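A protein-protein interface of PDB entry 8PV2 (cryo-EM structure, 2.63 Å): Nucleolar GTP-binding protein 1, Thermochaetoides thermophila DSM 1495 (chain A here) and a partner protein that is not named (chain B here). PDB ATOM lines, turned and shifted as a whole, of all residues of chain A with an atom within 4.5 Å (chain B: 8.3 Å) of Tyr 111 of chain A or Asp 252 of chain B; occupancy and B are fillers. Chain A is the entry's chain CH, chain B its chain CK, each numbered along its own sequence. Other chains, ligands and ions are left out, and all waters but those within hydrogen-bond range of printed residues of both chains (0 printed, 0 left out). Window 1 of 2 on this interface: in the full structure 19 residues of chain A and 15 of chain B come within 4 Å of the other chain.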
ATOM      1  N   ILE A 107       5.372  12.615 -32.078  1.00  0.00           N
ATOM      2  CA  ILE A 107       4.862  12.799 -30.719  1.00  0.00           C
ATOM      3  C   ILE A 107       5.461  11.761 -29.779  1.00  0.00           C
ATOM      4  O   ILE A 107       5.843  12.070 -28.640  1.00  0.00           O
ATOM      5  CB  ILE A 107       3.324  12.745 -30.725  1.00  0.00           C
ATOM      6  CG1 ILE A 107       2.760  14.067 -31.231  1.00  0.00           C
ATOM      7  CG2 ILE A 107       2.762  12.427 -29.352  1.00  0.00           C
ATOM      8  CD1 ILE A 107       1.277  14.063 -31.355  1.00  0.00           C
ATOM      9  N   SER A 108       5.566  10.518 -30.254  1.00  0.00           N
ATOM     10  CA  SER A 108       6.150   9.456 -29.442  1.00  0.00           C
ATOM     11  C   SER A 108       7.605   9.745 -29.104  1.00  0.00           C
ATOM     12  O   SER A 108       8.027   9.574 -27.955  1.00  0.00           O
ATOM     13  CB  SER A 108       6.030   8.126 -30.168  1.00  0.00           C
ATOM     14  OG  SER A 108       6.585   7.077 -29.401  1.00  0.00           O
ATOM     15  N   ARG A 109       8.383  10.203 -30.091  1.00  0.00           N
ATOM     16  CA  ARG A 109       9.785  10.523 -29.828  1.00  0.00           C
ATOM     17  C   ARG A 109       9.925  11.671 -28.835  1.00  0.00           C
ATOM     18  O   ARG A 109      10.760  11.607 -27.921  1.00  0.00           O
ATOM     19  CB  ARG A 109      10.510  10.854 -31.127  1.00  0.00           C
ATOM     20  CG  ARG A 109      10.695   9.677 -32.047  1.00  0.00           C
ATOM     21  CD  ARG A 109      11.730   9.985 -33.097  1.00  0.00           C
ATOM     22  NE  ARG A 109      11.480  11.271 -33.732  1.00  0.00           N
ATOM     23  CZ  ARG A 109      10.805  11.432 -34.861  1.00  0.00           C
ATOM     24  NH1 ARG A 109      10.298  10.401 -35.514  1.00  0.00           N
ATOM     25  NH2 ARG A 109      10.635  12.658 -35.346  1.00  0.00           N
ATOM     26  N   ASP A 110       9.098  12.712 -28.981  1.00  0.00           N
ATOM     27  CA  ASP A 110       9.161  13.856 -28.071  1.00  0.00           C
ATOM     28  C   ASP A 110       8.826  13.457 -26.638  1.00  0.00           C
ATOM     29  O   ASP A 110       9.509  13.861 -25.687  1.00  0.00           O
ATOM     30  CB  ASP A 110       8.216  14.957 -28.543  1.00  0.00           C
ATOM     31  CG  ASP A 110       8.715  15.660 -29.780  1.00  0.00           C
ATOM     32  OD1 ASP A 110       9.947  15.727 -29.970  1.00  0.00           O
ATOM     33  OD2 ASP A 110       7.877  16.156 -30.561  1.00  0.00           O
ATOM     34  N   TYR A 111       7.779  12.652 -26.460  1.00  0.00           N
ATOM     35  CA  TYR A 111       7.387  12.316 -25.099  1.00  0.00           C
ATOM     36  C   TYR A 111       8.283  11.256 -24.473  1.00  0.00           C
ATOM     37  O   TYR A 111       8.450  11.258 -23.253  1.00  0.00           O
ATOM     38  CB  TYR A 111       5.921  11.902 -25.063  1.00  0.00           C
ATOM     39  CG  TYR A 111       5.034  13.114 -25.009  1.00  0.00           C
ATOM     40  CD1 TYR A 111       4.792  13.763 -23.808  1.00  0.00           C
ATOM     41  CD2 TYR A 111       4.467  13.636 -26.162  1.00  0.00           C
ATOM     42  CE1 TYR A 111       3.998  14.881 -23.756  1.00  0.00           C
ATOM     43  CE2 TYR A 111       3.672  14.756 -26.117  1.00  0.00           C
ATOM     44  CZ  TYR A 111       3.443  15.374 -24.913  1.00  0.00           C
ATOM     45  OH  TYR A 111       2.648  16.488 -24.868  1.00  0.00           O
ATOM     46  N   VAL A 112       8.902  10.382 -25.270  1.00  0.00           N
ATOM     47  CA  VAL A 112       9.951   9.515 -24.740  1.00  0.00           C
ATOM     48  C   VAL A 112      11.138  10.345 -24.257  1.00  0.00           C
ATOM     49  O   VAL A 112      11.698  10.098 -23.173  1.00  0.00           O
ATOM     50  CB  VAL A 112      10.360   8.479 -25.803  1.00  0.00           C
ATOM     51  CG1 VAL A 112      11.685   7.841 -25.468  1.00  0.00           C
ATOM     52  CG2 VAL A 112       9.299   7.404 -25.907  1.00  0.00           C
ATOM     53  N   ARG A 113      11.508  11.370 -25.030  1.00  0.00           N
ATOM     54  CA  ARG A 113      12.605  12.244 -24.635  1.00  0.00           C
ATOM     55  C   ARG A 113      12.292  12.998 -23.343  1.00  0.00           C
ATOM     56  O   ARG A 113      13.184  13.225 -22.522  1.00  0.00           O
ATOM     57  CB  ARG A 113      12.919  13.212 -25.773  1.00  0.00           C
ATOM     58  CG  ARG A 113      14.290  13.836 -25.699  1.00  0.00           C
ATOM     59  CD  ARG A 113      14.553  14.768 -26.865  1.00  0.00           C
ATOM     60  NE  ARG A 113      14.452  14.116 -28.164  1.00  0.00           N
ATOM     61  CZ  ARG A 113      13.491  14.347 -29.046  1.00  0.00           C
ATOM     62  NH1 ARG A 113      12.518  15.205 -28.797  1.00  0.00           N
ATOM     63  NH2 ARG A 113      13.506  13.703 -30.207  1.00  0.00           N
ATOM     64  N   LEU A 114      11.031  13.401 -23.148  1.00  0.00           N
ATOM     65  CA  LEU A 114      10.665  14.079 -21.900  1.00  0.00           C
ATOM     66  C   LEU A 114      10.592  13.104 -20.724  1.00  0.00           C
ATOM     67  O   LEU A 114      10.933  13.454 -19.580  1.00  0.00           O
ATOM     68  CB  LEU A 114       9.333  14.805 -22.064  1.00  0.00           C
ATOM     69  CG  LEU A 114       9.281  15.966 -23.055  1.00  0.00           C
ATOM     70  CD1 LEU A 114       7.871  16.480 -23.170  1.00  0.00           C
ATOM     71  CD2 LEU A 114      10.224  17.075 -22.649  1.00  0.00           C
ATOM     72  N   LEU A 115      10.133  11.878 -20.985  1.00  0.00           N
ATOM     73  CA  LEU A 115      10.048  10.873 -19.936  1.00  0.00           C
ATOM     74  C   LEU A 115      11.424  10.461 -19.446  1.00  0.00           C
ATOM     75  O   LEU A 115      11.552   9.955 -18.328  1.00  0.00           O
ATOM     76  CB  LEU A 115       9.281   9.659 -20.446  1.00  0.00           C
ATOM     77  CG  LEU A 115       7.764   9.782 -20.397  1.00  0.00           C
ATOM     78  CD1 LEU A 115       7.125   8.643 -21.155  1.00  0.00           C
ATOM     79  CD2 LEU A 115       7.298   9.815 -18.960  1.00  0.00           C
ATOM     80  N   LEU A 127       2.660  12.958 -18.498  1.00  0.00           N
ATOM     81  CA  LEU A 127       3.294  12.928 -19.814  1.00  0.00           C
ATOM     82  C   LEU A 127       2.764  11.786 -20.671  1.00  0.00           C
ATOM     83  O   LEU A 127       2.558  11.955 -21.881  1.00  0.00           O
ATOM     84  CB  LEU A 127       4.809  12.837 -19.670  1.00  0.00           C
ATOM     85  CG  LEU A 127       5.494  14.134 -19.256  1.00  0.00           C
ATOM     86  CD1 LEU A 127       6.954  13.899 -18.950  1.00  0.00           C
ATOM     87  CD2 LEU A 127       5.332  15.175 -20.339  1.00  0.00           C
ATOM     88  N   ALA A 130      -0.666  12.840 -21.824  1.00  0.00           N
ATOM     89  CA  ALA A 130      -0.531  13.853 -22.865  1.00  0.00           C
ATOM     90  C   ALA A 130      -0.196  13.226 -24.211  1.00  0.00           C
ATOM     91  O   ALA A 130      -0.803  13.567 -25.235  1.00  0.00           O
ATOM     92  CB  ALA A 130       0.538  14.868 -22.468  1.00  0.00           C
ATOM     93  N   ALA A 131       0.756  12.287 -24.218  1.00  0.00           N
ATOM     94  CA  ALA A 131       1.134  11.605 -25.453  1.00  0.00           C
ATOM     95  C   ALA A 131      -0.041  10.844 -26.056  1.00  0.00           C
ATOM     96  O   ALA A 131      -0.359  11.010 -27.241  1.00  0.00           O
ATOM     97  CB  ALA A 131       2.304  10.660 -25.188  1.00  0.00           C
ATOM     98  N   ARG A 134      -2.818  13.166 -27.410  1.00  0.00           N
ATOM     99  CA  ARG A 134      -2.482  13.802 -28.682  1.00  0.00           C
ATOM    100  C   ARG A 134      -2.556  12.813 -29.842  1.00  0.00           C
ATOM    101  O   ARG A 134      -2.999  13.173 -30.944  1.00  0.00           O
ATOM    102  CB  ARG A 134      -1.108  14.457 -28.586  1.00  0.00           C
ATOM    103  CG  ARG A 134      -1.128  15.686 -27.714  1.00  0.00           C
ATOM    104  CD  ARG A 134       0.196  16.400 -27.641  1.00  0.00           C
ATOM    105  NE  ARG A 134       0.624  16.908 -28.933  1.00  0.00           N
ATOM    106  CZ  ARG A 134       1.654  17.723 -29.106  1.00  0.00           C
ATOM    107  NH1 ARG A 134       2.338  18.197 -28.080  1.00  0.00           N
ATOM    108  NH2 ARG A 134       2.011  18.061 -30.338  1.00  0.00           N
ATOM    109  N   PRO B 154      11.109  22.724 -18.038  1.00  0.00           N
ATOM    110  CA  PRO B 154      11.429  23.286 -19.356  1.00  0.00           C
ATOM    111  C   PRO B 154      12.075  24.657 -19.245  1.00  0.00           C
ATOM    112  O   PRO B 154      11.724  25.460 -18.381  1.00  0.00           O
ATOM    113  CB  PRO B 154      10.063  23.372 -20.039  1.00  0.00           C
ATOM    114  CG  PRO B 154       9.264  22.338 -19.396  1.00  0.00           C
ATOM    115  CD  PRO B 154       9.695  22.318 -17.967  1.00  0.00           C
ATOM    116  N   GLY B 176      16.755  18.191 -24.410  1.00  0.00           N
ATOM    117  CA  GLY B 176      15.419  17.659 -24.578  1.00  0.00           C
ATOM    118  C   GLY B 176      14.343  18.423 -23.843  1.00  0.00           C
ATOM    119  O   GLY B 176      13.160  18.140 -24.051  1.00  0.00           O
ATOM    120  N   TYR B 179      12.715  24.732 -25.063  1.00  0.00           N
ATOM    121  CA  TYR B 179      11.586  25.087 -25.904  1.00  0.00           C
ATOM    122  C   TYR B 179      11.853  26.400 -26.618  1.00  0.00           C
ATOM    123  O   TYR B 179      12.590  27.256 -26.125  1.00  0.00           O
ATOM    124  CB  TYR B 179      10.301  25.214 -25.092  1.00  0.00           C
ATOM    125  CG  TYR B 179       9.694  23.892 -24.721  1.00  0.00           C
ATOM    126  CD1 TYR B 179      10.178  23.167 -23.648  1.00  0.00           C
ATOM    127  CD2 TYR B 179       8.647  23.359 -25.456  1.00  0.00           C
ATOM    128  CE1 TYR B 179       9.634  21.956 -23.309  1.00  0.00           C
ATOM    129  CE2 TYR B 179       8.094  22.147 -25.124  1.00  0.00           C
ATOM    130  CZ  TYR B 179       8.592  21.450 -24.048  1.00  0.00           C
ATOM    131  OH  TYR B 179       8.052  20.239 -23.703  1.00  0.00           O
ATOM    132  N   ILE B 245       2.411  32.284 -18.903  1.00  0.00           N
ATOM    133  CA  ILE B 245       2.231  30.848 -19.060  1.00  0.00           C
ATOM    134  C   ILE B 245       1.122  30.378 -18.132  1.00  0.00           C
ATOM    135  O   ILE B 245       1.160  30.615 -16.918  1.00  0.00           O
ATOM    136  CB  ILE B 245       3.546  30.112 -18.783  1.00  0.00           C
ATOM    137  CG1 ILE B 245       4.588  30.498 -19.828  1.00  0.00           C
ATOM    138  CG2 ILE B 245       3.326  28.614 -18.765  1.00  0.00           C
ATOM    139  CD1 ILE B 245       5.932  29.888 -19.593  1.00  0.00           C
ATOM    140  N   THR B 246       0.130  29.700 -18.699  1.00  0.00           N
ATOM    141  CA  THR B 246      -1.067  29.310 -17.975  1.00  0.00           C
ATOM    142  C   THR B 246      -1.170  27.816 -17.721  1.00  0.00           C
ATOM    143  O   THR B 246      -2.163  27.373 -17.139  1.00  0.00           O
ATOM    144  CB  THR B 246      -2.307  29.784 -18.732  1.00  0.00           C
ATOM    145  OG1 THR B 246      -2.264  29.296 -20.075  1.00  0.00           O
ATOM    146  CG2 THR B 246      -2.355  31.289 -18.753  1.00  0.00           C
ATOM    147  N   ASN B 247      -0.180  27.029 -18.122  1.00  0.00           N
ATOM    148  CA  ASN B 247      -0.211  25.590 -17.925  1.00  0.00           C
ATOM    149  C   ASN B 247       1.053  25.153 -17.198  1.00  0.00           C
ATOM    150  O   ASN B 247       1.898  25.971 -16.828  1.00  0.00           O
ATOM    151  CB  ASN B 247      -0.374  24.857 -19.263  1.00  0.00           C
ATOM    152  CG  ASN B 247       0.896  24.831 -20.083  1.00  0.00           C
ATOM    153  OD1 ASN B 247       1.612  25.821 -20.176  1.00  0.00           O
ATOM    154  ND2 ASN B 247       1.172  23.697 -20.700  1.00  0.00           N
ATOM    155  N   ASN B 248       1.168  23.845 -16.979  1.00  0.00           N
ATOM    156  CA  ASN B 248       2.354  23.232 -16.391  1.00  0.00           C
ATOM    157  C   ASN B 248       3.130  22.520 -17.487  1.00  0.00           C
ATOM    158  O   ASN B 248       2.812  21.369 -17.821  1.00  0.00           O
ATOM    159  CB  ASN B 248       1.965  22.248 -15.285  1.00  0.00           C
ATOM    160  CG  ASN B 248       1.437  22.941 -14.054  1.00  0.00           C
ATOM    161  OD1 ASN B 248       2.138  23.728 -13.424  1.00  0.00           O
ATOM    162  ND2 ASN B 248       0.192  22.658 -13.705  1.00  0.00           N
ATOM    163  N   PRO B 249       4.144  23.159 -18.078  1.00  0.00           N
ATOM    164  CA  PRO B 249       4.803  22.570 -19.254  1.00  0.00           C
ATOM    165  C   PRO B 249       5.562  21.289 -18.969  1.00  0.00           C
ATOM    166  O   PRO B 249       5.687  20.451 -19.869  1.00  0.00           O
ATOM    167  CB  PRO B 249       5.740  23.692 -19.718  1.00  0.00           C
ATOM    168  CG  PRO B 249       5.185  24.932 -19.102  1.00  0.00           C
ATOM    169  CD  PRO B 249       4.662  24.504 -17.785  1.00  0.00           C
ATOM    170  N   GLU B 250       6.059  21.102 -17.742  1.00  0.00           N
ATOM    171  CA  GLU B 250       6.801  19.888 -17.430  1.00  0.00           C
ATOM    172  C   GLU B 250       5.887  18.671 -17.398  1.00  0.00           C
ATOM    173  O   GLU B 250       6.329  17.556 -17.688  1.00  0.00           O
ATOM    174  CB  GLU B 250       7.546  20.045 -16.097  1.00  0.00           C
ATOM    175  CG  GLU B 250       6.685  19.996 -14.848  1.00  0.00           C
ATOM    176  CD  GLU B 250       6.049  21.326 -14.497  1.00  0.00           C
ATOM    177  OE1 GLU B 250       6.298  22.325 -15.200  1.00  0.00           O
ATOM    178  OE2 GLU B 250       5.288  21.367 -13.510  1.00  0.00           O
ATOM    179  N   ASN B 251       4.609  18.869 -17.081  1.00  0.00           N
ATOM    180  CA  ASN B 251       3.622  17.804 -17.108  1.00  0.00           C
ATOM    181  C   ASN B 251       2.911  17.709 -18.443  1.00  0.00           C
ATOM    182  O   ASN B 251       2.371  16.649 -18.771  1.00  0.00           O
ATOM    183  CB  ASN B 251       2.572  18.025 -16.017  1.00  0.00           C
ATOM    184  CG  ASN B 251       3.155  17.970 -14.635  1.00  0.00           C
ATOM    185  OD1 ASN B 251       4.289  17.544 -14.447  1.00  0.00           O
ATOM    186  ND2 ASN B 251       2.388  18.415 -13.654  1.00  0.00           N
ATOM    187  N   ASP B 252       2.921  18.792 -19.213  1.00  0.00           N
ATOM    188  CA  ASP B 252       2.097  18.925 -20.399  1.00  0.00           C
ATOM    189  C   ASP B 252       2.835  18.618 -21.692  1.00  0.00           C
ATOM    190  O   ASP B 252       2.197  18.203 -22.663  1.00  0.00           O
ATOM    191  CB  ASP B 252       1.552  20.350 -20.465  1.00  0.00           C
ATOM    192  CG  ASP B 252       0.261  20.507 -19.719  1.00  0.00           C
ATOM    193  OD1 ASP B 252      -0.515  21.404 -20.086  1.00  0.00           O
ATOM    194  OD2 ASP B 252       0.006  19.728 -18.779  1.00  0.00           O
ATOM    195  N   GLY B 253       4.146  18.825 -21.736  1.00  0.00           N
ATOM    196  CA  GLY B 253       4.875  18.659 -22.972  1.00  0.00           C
ATOM    197  C   GLY B 253       4.737  19.800 -23.949  1.00  0.00           C
ATOM    198  O   GLY B 253       5.173  19.668 -25.097  1.00  0.00           O
ATOM    199  N   CYS B 254       4.141  20.914 -23.533  1.00  0.00           N
ATOM    200  CA  CYS B 254       3.963  22.078 -24.383  1.00  0.00           C
ATOM    201  C   CYS B 254       3.836  23.301 -23.491  1.00  0.00           C
ATOM    202  O   CYS B 254       3.624  23.189 -22.284  1.00  0.00           O
ATOM    203  CB  CYS B 254       2.729  21.946 -25.279  1.00  0.00           C
ATOM    204  SG  CYS B 254       1.169  21.835 -24.381  1.00  0.00           S
ATOM    205  N   VAL B 255       3.967  24.475 -24.097  1.00  0.00           N
ATOM    206  CA  VAL B 255       3.795  25.742 -23.401  1.00  0.00           C
ATOM    207  C   VAL B 255       2.508  26.378 -23.900  1.00  0.00           C
ATOM    208  O   VAL B 255       2.342  26.596 -25.104  1.00  0.00           O
ATOM    209  CB  VAL B 255       4.992  26.681 -23.613  1.00  0.00           C
ATOM    210  CG1 VAL B 255       4.799  27.963 -22.833  1.00  0.00           C
ATOM    211  CG2 VAL B 255       6.285  26.002 -23.209  1.00  0.00           C
ATOM    212  N   ASN B 256       1.595  26.658 -22.980  1.00  0.00           N
ATOM    213  CA  ASN B 256       0.381  27.405 -23.264  1.00  0.00           C
ATOM    214  C   ASN B 256       0.454  28.752 -22.563  1.00  0.00           C
ATOM    215  O   ASN B 256       0.745  28.821 -21.369  1.00  0.00           O
ATOM    216  CB  ASN B 256      -0.862  26.648 -22.802  1.00  0.00           C
ATOM    217  CG  ASN B 256      -1.080  25.373 -23.567  1.00  0.00           C
ATOM    218  OD1 ASN B 256      -0.686  25.257 -24.722  1.00  0.00           O
ATOM    219  ND2 ASN B 256      -1.698  24.400 -22.924  1.00  0.00           N
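OH of Tyr 111 of chain A lies within hydrogen-bond range of O of Asp 252 of chain B.
OD1 of Asp 110 of chain A lies within salt-bridge range of NH1 of Arg 113 of chain A, 2.9 Å away.
O of Gly 253 of chain B sits at hydrogen-bond distance from OH of Tyr 179 of chain B.
The side-chain amide nitrogen (ND2) of Asn 247 of chain B is in hydrogen-bond range of the side-chain carboxylate (OD1) of Asp 252 of chain B.
Among the printed residues, merely in contact across the chains: Leu 114 of chain A with Gly 176 of chain B (3.4 Å), Tyr 111 of chain A with Gly 253 of chain B (3.6 Å), Leu 127 of chain A with Asn 251 of chain B (3.7 Å), Leu 127 of chain A with Glu 250 of chain B (3.7 Å), Leu 114 of chain A with Gly 253 of chain B (3.7 Å), Ala 130 of chain A with Asp 252 of chain B (3.7 Å), Arg 113 of chain A with Gly 176 of chain B (3.8 Å) and Leu 114 of chain A with Tyr 179 of chain B (3.8 Å).
Asp 252 of chain B touches two residues of chain A.
Of the printed residues of chain B, Arg 113 of chain A touches Gly 176 (3.8 Å).
Printed residues of chain B within 4 Å of Ala 130 of chain A: Asp 252 (3.7 Å).
Of the printed residues of chain A, Tyr 179 of chain B touches Leu 114 (3.8 Å).
Of the printed residues of chain B, Leu 127 of chain A touches Glu 250 (3.7 Å) and Asn 251 (3.7 Å).
Of the printed residues of chain A, Gly 253 of chain B touches Tyr 111 and Leu 114.
The nearest printed residue of chain A that does not touch Asp 252 of chain B is Leu 127 of chain A (4.5 Å).
Of the 13 printed residues of chain A, 5 touch a printed residue of chain B.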
